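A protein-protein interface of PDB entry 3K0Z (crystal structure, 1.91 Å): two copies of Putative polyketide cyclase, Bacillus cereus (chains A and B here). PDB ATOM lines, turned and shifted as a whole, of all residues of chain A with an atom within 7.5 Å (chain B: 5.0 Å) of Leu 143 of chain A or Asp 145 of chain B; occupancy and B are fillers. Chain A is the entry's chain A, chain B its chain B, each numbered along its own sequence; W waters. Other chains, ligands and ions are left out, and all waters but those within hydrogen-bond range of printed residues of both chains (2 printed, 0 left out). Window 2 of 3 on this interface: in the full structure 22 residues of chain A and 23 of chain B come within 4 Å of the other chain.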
ATOM      1  N   THR A  67      27.103   0.136   1.023  1.00  0.00           N
ATOM      2  CA  THR A  67      27.833   0.871   2.053  1.00  0.00           C
ATOM      3  C   THR A  67      26.920   1.034   3.286  1.00  0.00           C
ATOM      4  O   THR A  67      26.580   2.127   3.701  1.00  0.00           O
ATOM      5  CB  THR A  67      28.234   2.229   1.475  1.00  0.00           C
ATOM      6  OG1 THR A  67      27.059   2.886   0.989  1.00  0.00           O
ATOM      7  CG2 THR A  67      29.243   2.102   0.296  1.00  0.00           C
ATOM      8  N   LEU A  68      26.560  -0.096   3.874  1.00  0.00           N
ATOM      9  CA  LEU A  68      25.471  -0.160   4.822  1.00  0.00           C
ATOM     10  C   LEU A  68      25.963   0.360   6.148  1.00  0.00           C
ATOM     11  O   LEU A  68      26.932  -0.174   6.650  1.00  0.00           O
ATOM     12  CB  LEU A  68      25.033  -1.620   4.872  1.00  0.00           C
ATOM     13  CG  LEU A  68      23.709  -2.097   5.387  1.00  0.00           C
ATOM     14  CD1 LEU A  68      22.500  -1.456   4.614  1.00  0.00           C
ATOM     15  CD2 LEU A  68      23.752  -3.635   5.308  1.00  0.00           C
ATOM     16  N   PRO A  69      25.363   1.454   6.691  1.00  0.00           N
ATOM     17  CA  PRO A  69      25.765   1.913   8.030  1.00  0.00           C
ATOM     18  C   PRO A  69      25.690   0.810   9.093  1.00  0.00           C
ATOM     19  O   PRO A  69      24.876  -0.122   8.962  1.00  0.00           O
ATOM     20  CB  PRO A  69      24.764   3.026   8.322  1.00  0.00           C
ATOM     21  CG  PRO A  69      24.396   3.550   7.005  1.00  0.00           C
ATOM     22  CD  PRO A  69      24.341   2.345   6.121  1.00  0.00           C
ATOM     23  N   ALA A 109      23.812  12.166  -6.210  1.00  0.00           N
ATOM     24  CA  ALA A 109      23.066  13.195  -5.498  1.00  0.00           C
ATOM     25  C   ALA A 109      23.897  13.745  -4.360  1.00  0.00           C
ATOM     26  O   ALA A 109      24.513  12.952  -3.609  1.00  0.00           O
ATOM     27  CB  ALA A 109      21.693  12.631  -4.930  1.00  0.00           C
ATOM     28  N   LEU A 111      23.214  15.881  -1.008  1.00  0.00           N
ATOM     29  CA  LEU A 111      22.091  16.238  -0.133  1.00  0.00           C
ATOM     30  C   LEU A 111      22.451  17.166   1.008  1.00  0.00           C
ATOM     31  O   LEU A 111      23.621  17.220   1.421  1.00  0.00           O
ATOM     32  CB  LEU A 111      21.498  14.962   0.470  1.00  0.00           C
ATOM     33  CG  LEU A 111      20.959  13.855  -0.469  1.00  0.00           C
ATOM     34  CD1 LEU A 111      20.100  14.406  -1.703  1.00  0.00           C
ATOM     35  CD2 LEU A 111      22.049  12.851  -0.926  1.00  0.00           C
ATOM     36  N   PHE A 113      20.856  18.023   4.878  1.00  0.00           N
ATOM     37  CA  PHE A 113      19.906  17.645   5.915  1.00  0.00           C
ATOM     38  C   PHE A 113      19.960  18.732   6.972  1.00  0.00           C
ATOM     39  O   PHE A 113      21.044  19.020   7.517  1.00  0.00           O
ATOM     40  CB  PHE A 113      20.293  16.320   6.562  1.00  0.00           C
ATOM     41  CG  PHE A 113      20.033  15.129   5.706  1.00  0.00           C
ATOM     42  CD1 PHE A 113      18.787  14.487   5.743  1.00  0.00           C
ATOM     43  CD2 PHE A 113      21.026  14.631   4.875  1.00  0.00           C
ATOM     44  CE1 PHE A 113      18.544  13.380   4.938  1.00  0.00           C
ATOM     45  CE2 PHE A 113      20.792  13.508   4.070  1.00  0.00           C
ATOM     46  CZ  PHE A 113      19.540  12.902   4.092  1.00  0.00           C
ATOM     47  N   PHE A 124      23.925  19.032   8.124  1.00  0.00           N
ATOM     48  CA  PHE A 124      24.983  18.171   7.621  1.00  0.00           C
ATOM     49  C   PHE A 124      24.645  17.738   6.213  1.00  0.00           C
ATOM     50  O   PHE A 124      23.484  17.807   5.793  1.00  0.00           O
ATOM     51  CB  PHE A 124      25.253  16.938   8.538  1.00  0.00           C
ATOM     52  CG  PHE A 124      24.119  15.938   8.583  1.00  0.00           C
ATOM     53  CD1 PHE A 124      23.049  16.121   9.473  1.00  0.00           C
ATOM     54  CD2 PHE A 124      24.107  14.830   7.746  1.00  0.00           C
ATOM     55  CE1 PHE A 124      21.994  15.220   9.500  1.00  0.00           C
ATOM     56  CE2 PHE A 124      23.052  13.919   7.789  1.00  0.00           C
ATOM     57  CZ  PHE A 124      22.000  14.113   8.681  1.00  0.00           C
ATOM     58  N   PHE A 125      25.660  17.274   5.503  1.00  0.00           N
ATOM     59  CA  PHE A 125      25.483  16.839   4.128  1.00  0.00           C
ATOM     60  C   PHE A 125      25.762  15.354   3.857  1.00  0.00           C
ATOM     61  O   PHE A 125      26.320  14.632   4.690  1.00  0.00           O
ATOM     62  CB  PHE A 125      26.290  17.732   3.201  1.00  0.00           C
ATOM     63  CG  PHE A 125      27.724  17.369   3.101  1.00  0.00           C
ATOM     64  CD1 PHE A 125      28.629  17.849   4.008  1.00  0.00           C
ATOM     65  CD2 PHE A 125      28.189  16.566   2.054  1.00  0.00           C
ATOM     66  CE1 PHE A 125      29.975  17.535   3.920  1.00  0.00           C
ATOM     67  CE2 PHE A 125      29.536  16.250   1.953  1.00  0.00           C
ATOM     68  CZ  PHE A 125      30.428  16.747   2.934  1.00  0.00           C
ATOM     69  N   ALA A 126      25.329  14.896   2.678  1.00  0.00           N
ATOM     70  CA  ALA A 126      25.555  13.509   2.259  1.00  0.00           C
ATOM     71  C   ALA A 126      25.816  13.519   0.746  1.00  0.00           C
ATOM     72  O   ALA A 126      25.419  14.466   0.037  1.00  0.00           O
ATOM     73  CB  ALA A 126      24.335  12.642   2.608  1.00  0.00           C
ATOM     74  N   ILE A 127      26.497  12.488   0.266  1.00  0.00           N
ATOM     75  CA  ILE A 127      26.639  12.234  -1.179  1.00  0.00           C
ATOM     76  C   ILE A 127      26.283  10.763  -1.439  1.00  0.00           C
ATOM     77  O   ILE A 127      26.774   9.863  -0.718  1.00  0.00           O
ATOM     78  CB  ILE A 127      28.072  12.513  -1.750  1.00  0.00           C
ATOM     79  CG1 ILE A 127      28.557  13.929  -1.405  1.00  0.00           C
ATOM     80  CG2 ILE A 127      28.024  12.299  -3.262  1.00  0.00           C
ATOM     81  CD1 ILE A 127      30.018  14.242  -1.781  1.00  0.00           C
ATOM     82  N   ASP A 128      25.434  10.523  -2.448  1.00  0.00           N
ATOM     83  CA  ASP A 128      24.989   9.186  -2.785  1.00  0.00           C
ATOM     84  C   ASP A 128      25.228   8.935  -4.245  1.00  0.00           C
ATOM     85  O   ASP A 128      25.051   9.836  -5.064  1.00  0.00           O
ATOM     86  CB  ASP A 128      23.483   8.999  -2.611  1.00  0.00           C
ATOM     87  CG  ASP A 128      22.969   9.226  -1.190  1.00  0.00           C
ATOM     88  OD1 ASP A 128      23.725   9.662  -0.274  1.00  0.00           O
ATOM     89  OD2 ASP A 128      21.764   8.927  -0.980  1.00  0.00           O
ATOM     90  N   ILE A 129      25.593   7.707  -4.568  1.00  0.00           N
ATOM     91  CA  ILE A 129      25.686   7.251  -5.951  1.00  0.00           C
ATOM     92  C   ILE A 129      24.609   6.162  -6.096  1.00  0.00           C
ATOM     93  O   ILE A 129      24.627   5.145  -5.382  1.00  0.00           O
ATOM     94  CB  ILE A 129      27.053   6.666  -6.302  1.00  0.00           C
ATOM     95  CG1 ILE A 129      28.126   7.767  -6.221  1.00  0.00           C
ATOM     96  CG2 ILE A 129      26.991   6.049  -7.718  1.00  0.00           C
ATOM     97  CD1 ILE A 129      29.548   7.233  -6.167  1.00  0.00           C
ATOM     98  N   ASP A 140      23.065   1.128  -4.261  1.00  0.00           N
ATOM     99  CA  ASP A 140      23.685   2.396  -4.028  1.00  0.00           C
ATOM    100  C   ASP A 140      24.928   2.303  -3.178  1.00  0.00           C
ATOM    101  O   ASP A 140      25.225   1.263  -2.576  1.00  0.00           O
ATOM    102  CB  ASP A 140      22.681   3.448  -3.523  1.00  0.00           C
ATOM    103  CG  ASP A 140      22.284   3.265  -2.058  1.00  0.00           C
ATOM    104  OD1 ASP A 140      22.462   2.172  -1.543  1.00  0.00           O
ATOM    105  OD2 ASP A 140      21.797   4.235  -1.416  1.00  0.00           O
ATOM    106  N   TRP A 141      25.634   3.423  -3.175  1.00  0.00           N
ATOM    107  CA  TRP A 141      26.841   3.687  -2.403  1.00  0.00           C
ATOM    108  C   TRP A 141      26.645   5.092  -1.883  1.00  0.00           C
ATOM    109  O   TRP A 141      26.467   6.028  -2.657  1.00  0.00           O
ATOM    110  CB  TRP A 141      28.093   3.654  -3.276  1.00  0.00           C
ATOM    111  CG  TRP A 141      28.336   2.399  -4.014  1.00  0.00           C
ATOM    112  CD1 TRP A 141      29.234   1.409  -3.689  1.00  0.00           C
ATOM    113  CD2 TRP A 141      27.778   2.019  -5.294  1.00  0.00           C
ATOM    114  NE1 TRP A 141      29.230   0.458  -4.656  1.00  0.00           N
ATOM    115  CE2 TRP A 141      28.351   0.803  -5.650  1.00  0.00           C
ATOM    116  CE3 TRP A 141      26.871   2.611  -6.166  1.00  0.00           C
ATOM    117  CZ2 TRP A 141      28.004   0.119  -6.833  1.00  0.00           C
ATOM    118  CZ3 TRP A 141      26.529   1.942  -7.344  1.00  0.00           C
ATOM    119  CH2 TRP A 141      27.078   0.697  -7.646  1.00  0.00           C
ATOM    120  N   HIS A 142      26.712   5.277  -0.569  1.00  0.00           N
ATOM    121  CA  HIS A 142      26.381   6.571  -0.027  1.00  0.00           C
ATOM    122  C   HIS A 142      27.141   6.825   1.254  1.00  0.00           C
ATOM    123  O   HIS A 142      27.631   5.893   1.932  1.00  0.00           O
ATOM    124  CB  HIS A 142      24.871   6.616   0.242  1.00  0.00           C
ATOM    125  CG  HIS A 142      24.424   5.662   1.302  1.00  0.00           C
ATOM    126  ND1 HIS A 142      24.230   6.045   2.612  1.00  0.00           N
ATOM    127  CD2 HIS A 142      24.156   4.334   1.251  1.00  0.00           C
ATOM    128  CE1 HIS A 142      23.832   5.001   3.316  1.00  0.00           C
ATOM    129  NE2 HIS A 142      23.788   3.948   2.516  1.00  0.00           N
ATOM    130  N   LEU A 143      27.236   8.098   1.596  1.00  0.00           N
ATOM    131  CA  LEU A 143      27.931   8.511   2.839  1.00  0.00           C
ATOM    132  C   LEU A 143      27.292   9.777   3.382  1.00  0.00           C
ATOM    133  O   LEU A 143      27.045  10.721   2.620  1.00  0.00           O
ATOM    134  CB  LEU A 143      29.390   8.742   2.475  1.00  0.00           C
ATOM    135  CG  LEU A 143      30.508   8.575   3.462  1.00  0.00           C
ATOM    136  CD1 LEU A 143      30.347   7.354   4.391  1.00  0.00           C
ATOM    137  CD2 LEU A 143      31.803   8.519   2.614  1.00  0.00           C
ATOM    138  N   GLU A 144      26.961   9.758   4.665  1.00  0.00           N
ATOM    139  CA  GLU A 144      26.374  10.909   5.356  1.00  0.00           C
ATOM    140  C   GLU A 144      27.465  11.376   6.261  1.00  0.00           C
ATOM    141  O   GLU A 144      28.252  10.550   6.744  1.00  0.00           O
ATOM    142  CB  GLU A 144      25.158  10.498   6.180  1.00  0.00           C
ATOM    143  CG  GLU A 144      23.952  10.050   5.356  1.00  0.00           C
ATOM    144  CD  GLU A 144      24.094   8.659   4.746  1.00  0.00           C
ATOM    145  OE1 GLU A 144      24.227   7.697   5.520  1.00  0.00           O
ATOM    146  OE2 GLU A 144      24.034   8.559   3.491  1.00  0.00           O
ATOM    147  N   ASP A 145      27.555  12.674   6.496  1.00  0.00           N
ATOM    148  CA  ASP A 145      28.645  13.195   7.366  1.00  0.00           C
ATOM    149  C   ASP A 145      28.236  13.006   8.835  1.00  0.00           C
ATOM    150  O   ASP A 145      27.873  13.944   9.517  1.00  0.00           O
ATOM    151  CB  ASP A 145      28.965  14.657   6.984  1.00  0.00           C
ATOM    152  CG  ASP A 145      30.170  15.222   7.723  1.00  0.00           C
ATOM    153  OD1 ASP A 145      30.815  14.483   8.493  1.00  0.00           O
ATOM    154  OD2 ASP A 145      30.461  16.418   7.519  1.00  0.00           O
ATOM    155  N   ASN A 146      28.311  11.743   9.286  1.00  0.00           N
ATOM    156  CA  ASN A 146      27.829  11.347  10.612  1.00  0.00           C
ATOM    157  C   ASN A 146      28.674  11.882  11.765  1.00  0.00           C
ATOM    158  O   ASN A 146      28.152  12.114  12.839  1.00  0.00           O
ATOM    159  CB  ASN A 146      27.684   9.818  10.727  1.00  0.00           C
ATOM    160  CG  ASN A 146      26.603   9.240   9.795  1.00  0.00           C
ATOM    161  OD1 ASN A 146      26.906   8.353   8.985  1.00  0.00           O
ATOM    162  ND2 ASN A 146      25.364   9.752   9.887  1.00  0.00           N
ATOM    163  N   LEU A 147      29.968  12.075  11.546  1.00  0.00           N
ATOM    164  CA  LEU A 147      30.811  12.655  12.587  1.00  0.00           C
ATOM    165  C   LEU A 147      30.307  14.101  12.896  1.00  0.00           C
ATOM    166  O   LEU A 147      30.119  14.472  14.065  1.00  0.00           O
ATOM    167  CB  LEU A 147      32.288  12.632  12.139  1.00  0.00           C
ATOM    168  CG  LEU A 147      33.358  13.054  13.147  1.00  0.00           C
ATOM    169  CD1 LEU A 147      33.315  12.193  14.395  1.00  0.00           C
ATOM    170  CD2 LEU A 147      34.771  13.014  12.518  1.00  0.00           C
ATOM    171  N   PHE B 124      38.866   2.533   4.523  1.00  0.00           N
ATOM    172  CA  PHE B 124      37.675   3.368   4.485  1.00  0.00           C
ATOM    173  C   PHE B 124      37.477   3.902   3.088  1.00  0.00           C
ATOM    174  O   PHE B 124      38.425   3.932   2.301  1.00  0.00           O
ATOM    175  CB  PHE B 124      37.775   4.512   5.519  1.00  0.00           C
ATOM    176  CG  PHE B 124      38.799   5.542   5.203  1.00  0.00           C
ATOM    177  CD1 PHE B 124      40.104   5.397   5.623  1.00  0.00           C
ATOM    178  CD2 PHE B 124      38.450   6.680   4.497  1.00  0.00           C
ATOM    179  CE1 PHE B 124      41.048   6.342   5.345  1.00  0.00           C
ATOM    180  CE2 PHE B 124      39.390   7.622   4.210  1.00  0.00           C
ATOM    181  CZ  PHE B 124      40.695   7.467   4.632  1.00  0.00           C
ATOM    182  N   PHE B 125      36.256   4.322   2.786  1.00  0.00           N
ATOM    183  CA  PHE B 125      35.924   4.843   1.472  1.00  0.00           C
ATOM    184  C   PHE B 125      35.545   6.317   1.529  1.00  0.00           C
ATOM    185  O   PHE B 125      35.393   6.912   2.600  1.00  0.00           O
ATOM    186  CB  PHE B 125      34.824   3.994   0.757  1.00  0.00           C
ATOM    187  CG  PHE B 125      33.410   4.269   1.212  1.00  0.00           C
ATOM    188  CD1 PHE B 125      32.933   3.744   2.374  1.00  0.00           C
ATOM    189  CD2 PHE B 125      32.550   5.053   0.439  1.00  0.00           C
ATOM    190  CE1 PHE B 125      31.623   4.004   2.791  1.00  0.00           C
ATOM    191  CE2 PHE B 125      31.253   5.285   0.847  1.00  0.00           C
ATOM    192  CZ  PHE B 125      30.812   4.773   2.018  1.00  0.00           C
ATOM    193  N   ALA B 126      35.434   6.896   0.339  1.00  0.00           N
ATOM    194  CA  ALA B 126      35.085   8.277   0.185  1.00  0.00           C
ATOM    195  C   ALA B 126      34.362   8.514  -1.108  1.00  0.00           C
ATOM    196  O   ALA B 126      34.418   7.706  -2.043  1.00  0.00           O
ATOM    197  CB  ALA B 126      36.307   9.140   0.246  1.00  0.00           C
ATOM    198  N   ILE B 127      33.641   9.634  -1.160  1.00  0.00           N
ATOM    199  CA  ILE B 127      32.970  10.035  -2.388  1.00  0.00           C
ATOM    200  C   ILE B 127      33.215  11.535  -2.559  1.00  0.00           C
ATOM    201  O   ILE B 127      33.030  12.310  -1.609  1.00  0.00           O
ATOM    202  CB  ILE B 127      31.435   9.771  -2.432  1.00  0.00           C
ATOM    203  CG1 ILE B 127      31.090   8.290  -2.193  1.00  0.00           C
ATOM    204  CG2 ILE B 127      30.880  10.247  -3.764  1.00  0.00           C
ATOM    205  CD1 ILE B 127      29.595   7.978  -2.001  1.00  0.00           C
ATOM    206  N   LEU B 143      33.542  13.772   0.865  1.00  0.00           N
ATOM    207  CA  LEU B 143      33.273  13.198   2.142  1.00  0.00           C
ATOM    208  C   LEU B 143      33.991  11.861   2.282  1.00  0.00           C
ATOM    209  O   LEU B 143      33.870  10.993   1.423  1.00  0.00           O
ATOM    210  CB  LEU B 143      31.765  12.979   2.314  1.00  0.00           C
ATOM    211  CG  LEU B 143      31.232  12.618   3.705  1.00  0.00           C
ATOM    212  CD1 LEU B 143      31.746  13.538   4.785  1.00  0.00           C
ATOM    213  CD2 LEU B 143      29.655  12.604   3.676  1.00  0.00           C
ATOM    214  N   GLU B 144      34.713  11.731   3.380  1.00  0.00           N
ATOM    215  CA  GLU B 144      35.391  10.494   3.771  1.00  0.00           C
ATOM    216  C   GLU B 144      34.570   9.880   4.914  1.00  0.00           C
ATOM    217  O   GLU B 144      33.851  10.590   5.623  1.00  0.00           O
ATOM    218  CB  GLU B 144      36.841  10.778   4.212  1.00  0.00           C
ATOM    219  CG  GLU B 144      37.748  11.322   3.107  1.00  0.00           C
ATOM    220  CD  GLU B 144      37.494  12.817   2.723  1.00  0.00           C
ATOM    221  OE1 GLU B 144      37.763  13.703   3.538  1.00  0.00           O
ATOM    222  OE2 GLU B 144      37.099  13.107   1.579  1.00  0.00           O
ATOM    223  N   ASP B 145      34.647   8.560   5.074  1.00  0.00           N
ATOM    224  CA  ASP B 145      33.940   7.892   6.143  1.00  0.00           C
ATOM    225  C   ASP B 145      34.766   8.038   7.442  1.00  0.00           C
ATOM    226  O   ASP B 145      35.444   7.097   7.898  1.00  0.00           O
ATOM    227  CB  ASP B 145      33.646   6.428   5.787  1.00  0.00           C
ATOM    228  CG  ASP B 145      32.762   5.749   6.819  1.00  0.00           C
ATOM    229  OD1 ASP B 145      32.390   6.435   7.805  1.00  0.00           O
ATOM    230  OD2 ASP B 145      32.466   4.548   6.663  1.00  0.00           O
ATOM    231  N   ASN B 146      34.677   9.245   8.012  1.00  0.00           N
ATOM    232  CA  ASN B 146      35.498   9.707   9.119  1.00  0.00           C
ATOM    233  C   ASN B 146      35.159   8.970  10.407  1.00  0.00           C
ATOM    234  O   ASN B 146      36.001   8.814  11.263  1.00  0.00           O
ATOM    235  CB  ASN B 146      35.354  11.249   9.327  1.00  0.00           C
ATOM    236  CG  ASN B 146      35.903  12.114   8.137  1.00  0.00           C
ATOM    237  OD1 ASN B 146      35.237  13.056   7.660  1.00  0.00           O
ATOM    238  ND2 ASN B 146      37.115  11.829   7.705  1.00  0.00           N
ATOM    239  N   LEU B 147      33.934   8.498  10.545  1.00  0.00           N
ATOM    240  CA  LEU B 147      33.580   7.760  11.750  1.00  0.00           C
ATOM    241  C   LEU B 147      34.258   6.403  11.703  1.00  0.00           C
ATOM    242  O   LEU B 147      34.824   5.967  12.715  1.00  0.00           O
ATOM    243  CB  LEU B 147      32.066   7.580  11.882  1.00  0.00           C
ATOM    244  CG  LEU B 147      31.492   7.423  13.278  1.00  0.00           C
ATOM    245  CD1 LEU B 147      31.703   8.713  14.123  1.00  0.00           C
ATOM    246  CD2 LEU B 147      30.021   7.092  13.165  1.00  0.00           C
ATOM    247  N   THR B 148      34.198   5.729  10.544  1.00  0.00           N
ATOM    248  CA  THR B 148      34.898   4.449  10.373  1.00  0.00           C
ATOM    249  C   THR B 148      36.407   4.637  10.606  1.00  0.00           C
ATOM    250  O   THR B 148      37.005   3.895  11.368  1.00  0.00           O
ATOM    251  CB  THR B 148      34.638   3.798   8.999  1.00  0.00           C
ATOM    252  OG1 THR B 148      33.242   3.510   8.851  1.00  0.00           O
ATOM    253  CG2 THR B 148      35.398   2.502   8.853  1.00  0.00           C
ATOM    254  N   LEU B 149      36.996   5.644   9.967  1.00  0.00           N
ATOM    255  CA  LEU B 149      38.401   5.936  10.139  1.00  0.00           C
ATOM    256  C   LEU B 149      38.779   6.181  11.584  1.00  0.00           C
ATOM    257  O   LEU B 149      39.731   5.561  12.056  1.00  0.00           O
ATOM    258  CB  LEU B 149      38.833   7.118   9.273  1.00  0.00           C
ATOM    259  CG  LEU B 149      40.280   7.600   9.383  1.00  0.00           C
ATOM    260  CD1 LEU B 149      41.248   6.432   9.140  1.00  0.00           C
ATOM    261  CD2 LEU B 149      40.566   8.806   8.489  1.00  0.00           C
HETATM  262  O   HOH W   1      30.794   9.800   6.803  1.00  0.00           O
HETATM  263  O   HOH W   2      33.359  14.767   9.301  1.00  0.00           O
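Phe 125 of chain A touches Leu 143 of chain B, and with the chains exchanged Leu 143 of chain A touches Phe 125 of chain B. Ile 127 of chain B touches its own counterpart, Ile 127 of chain A. Leu 143 of chain A touches Glu 144 of chain B, and with the chains exchanged Glu 144 of chain A touches Leu 143 of chain B. Leu 143 of chain A touches Asp 145 of chain B, and with the chains exchanged Asp 145 of chain A touches Leu 143 of chain B. Positions printed for both chains: 124, 125, 126, 127, 143, 144, 145, 146 and 147. Of the 13 pairs that touch across the chains among the printed residues, 9 have their exchanged pair printed and touching as well.
Leu 143 of chain A touches just these residues of chain B: Phe 125 (3.5 Å), Leu 143 (3.4 Å), Glu 144 (3.8 Å) and Asp 145 (3.7 Å). Of chain A, only Leu 143 comes within 4 Å of Asp 145 of chain B. Of the printed residues of chain B, Asp 145 of chain A touches Leu 143. Printed residues of chain A within 4 Å of Phe 125 of chain B: Thr 67, His 142 and Leu 143. Of the printed residues of chain B, Phe 125 of chain A touches Leu 143 (3.9 Å). Printed residues of chain B within 4 Å of Ile 127 of chain A: Ile 127. Of the printed residues of chain A, Ile 127 of chain B touches Ile 127 (3.6 Å) and Trp 141 (3.7 Å). Ala 126 of chain B touches none of the printed residues of chain A. Ala 126 of chain A touches none of the printed residues of chain B. The nearest residue of chain B that does not touch Leu 143 of chain A is Ala 126 of chain B (4.1 Å). The nearest printed residue of chain A that does not touch Asp 145 of chain B is Asn 146 of chain A (5.9 Å).
Of the 11 printed residues of chain B, 7 touch a printed residue of chain A. Of the 20 printed residues of chain A, 9 touch a printed residue of chain B. Printed residues of chain A that touch a printed residue of chain B: Thr 67, Phe 125, Ile 127, Trp 141, His 142, Leu 143, Glu 144, Asp 145 and Leu 147. Hydrophobic or aromatic side chains of chain A within 4 Å of the printed part of chain B: Phe 125, Ile 127, Leu 143 and Leu 147. Among the printed residues, 13 pairs touch across the chains. Among the printed residues, no Asp or Glu carboxylate lies within 4 Å of a Lys or Arg side-chain nitrogen of the other chain.
Water W1 lies within hydrogen-bond range of the backbone carbonyl oxygen (O) of Glu 144 of chain A (2.7 Å) and the backbone carbonyl oxygen (O) of Glu 144 of chain B (3.4 Å). Water W2 lies within hydrogen-bond range of the side-chain carboxylate (OD1) of Asp 145 of chain A (2.7 Å) and the side-chain amide oxygen (OD1) of Asn 146 of chain B (3.0 Å).
Among the printed residues, merely in contact across the chains: Thr 67 of chain A with Phe 125 of chain B, Phe 125 of chain A with Leu 143 of chain B, Ile 127 of chain A with Ile 127 of chain B, Trp 141 of chain A with Ile 127 of chain B, His 142 of chain A with Phe 125 of chain B, Leu 143 of chain A with Phe 125 of chain B, Leu 143 of chain A with Leu 143 of chain B, Leu 143 of chain A with Glu 144 of chain B, Leu 143 of chain A with Asp 145 of chain B, Glu 144 of chain A with Leu 143 of chain B, Asp 145 of chain A with Leu 143 of chain B, Leu 147 of chain A with Asn 146 of chain B and Leu 147 of chain A with Leu 147 of chain B.
The side-chain hydroxyl (OG1) of Thr 67 of chain A sits at hydrogen-bond distance from the backbone NH (N) of His 142 of chain A, 2.9 Å away. OD1 of Asn 146 of chain A lies close to O of Glu 144 of chain A (3.4 Å). O of Phe 125 of chain B sits at hydrogen-bond distance from N of Asp 145 of chain B, at 3.1 Å. The backbone NH (N) of Leu 143 of chain B lies within hydrogen-bond range of the backbone carbonyl oxygen (O) of Ile 127 of chain B (2.9 Å). The backbone carbonyl oxygen (O) of Glu 144 of chain B sits close to the side-chain amide oxygen (OD1) of Asn 146 of chain B (3.5 Å). The side-chain carboxylate (OD2) of Asp 145 of chain B lies within hydrogen-bond range of the side-chain hydroxyl (OG1) of Thr 148 of chain B.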
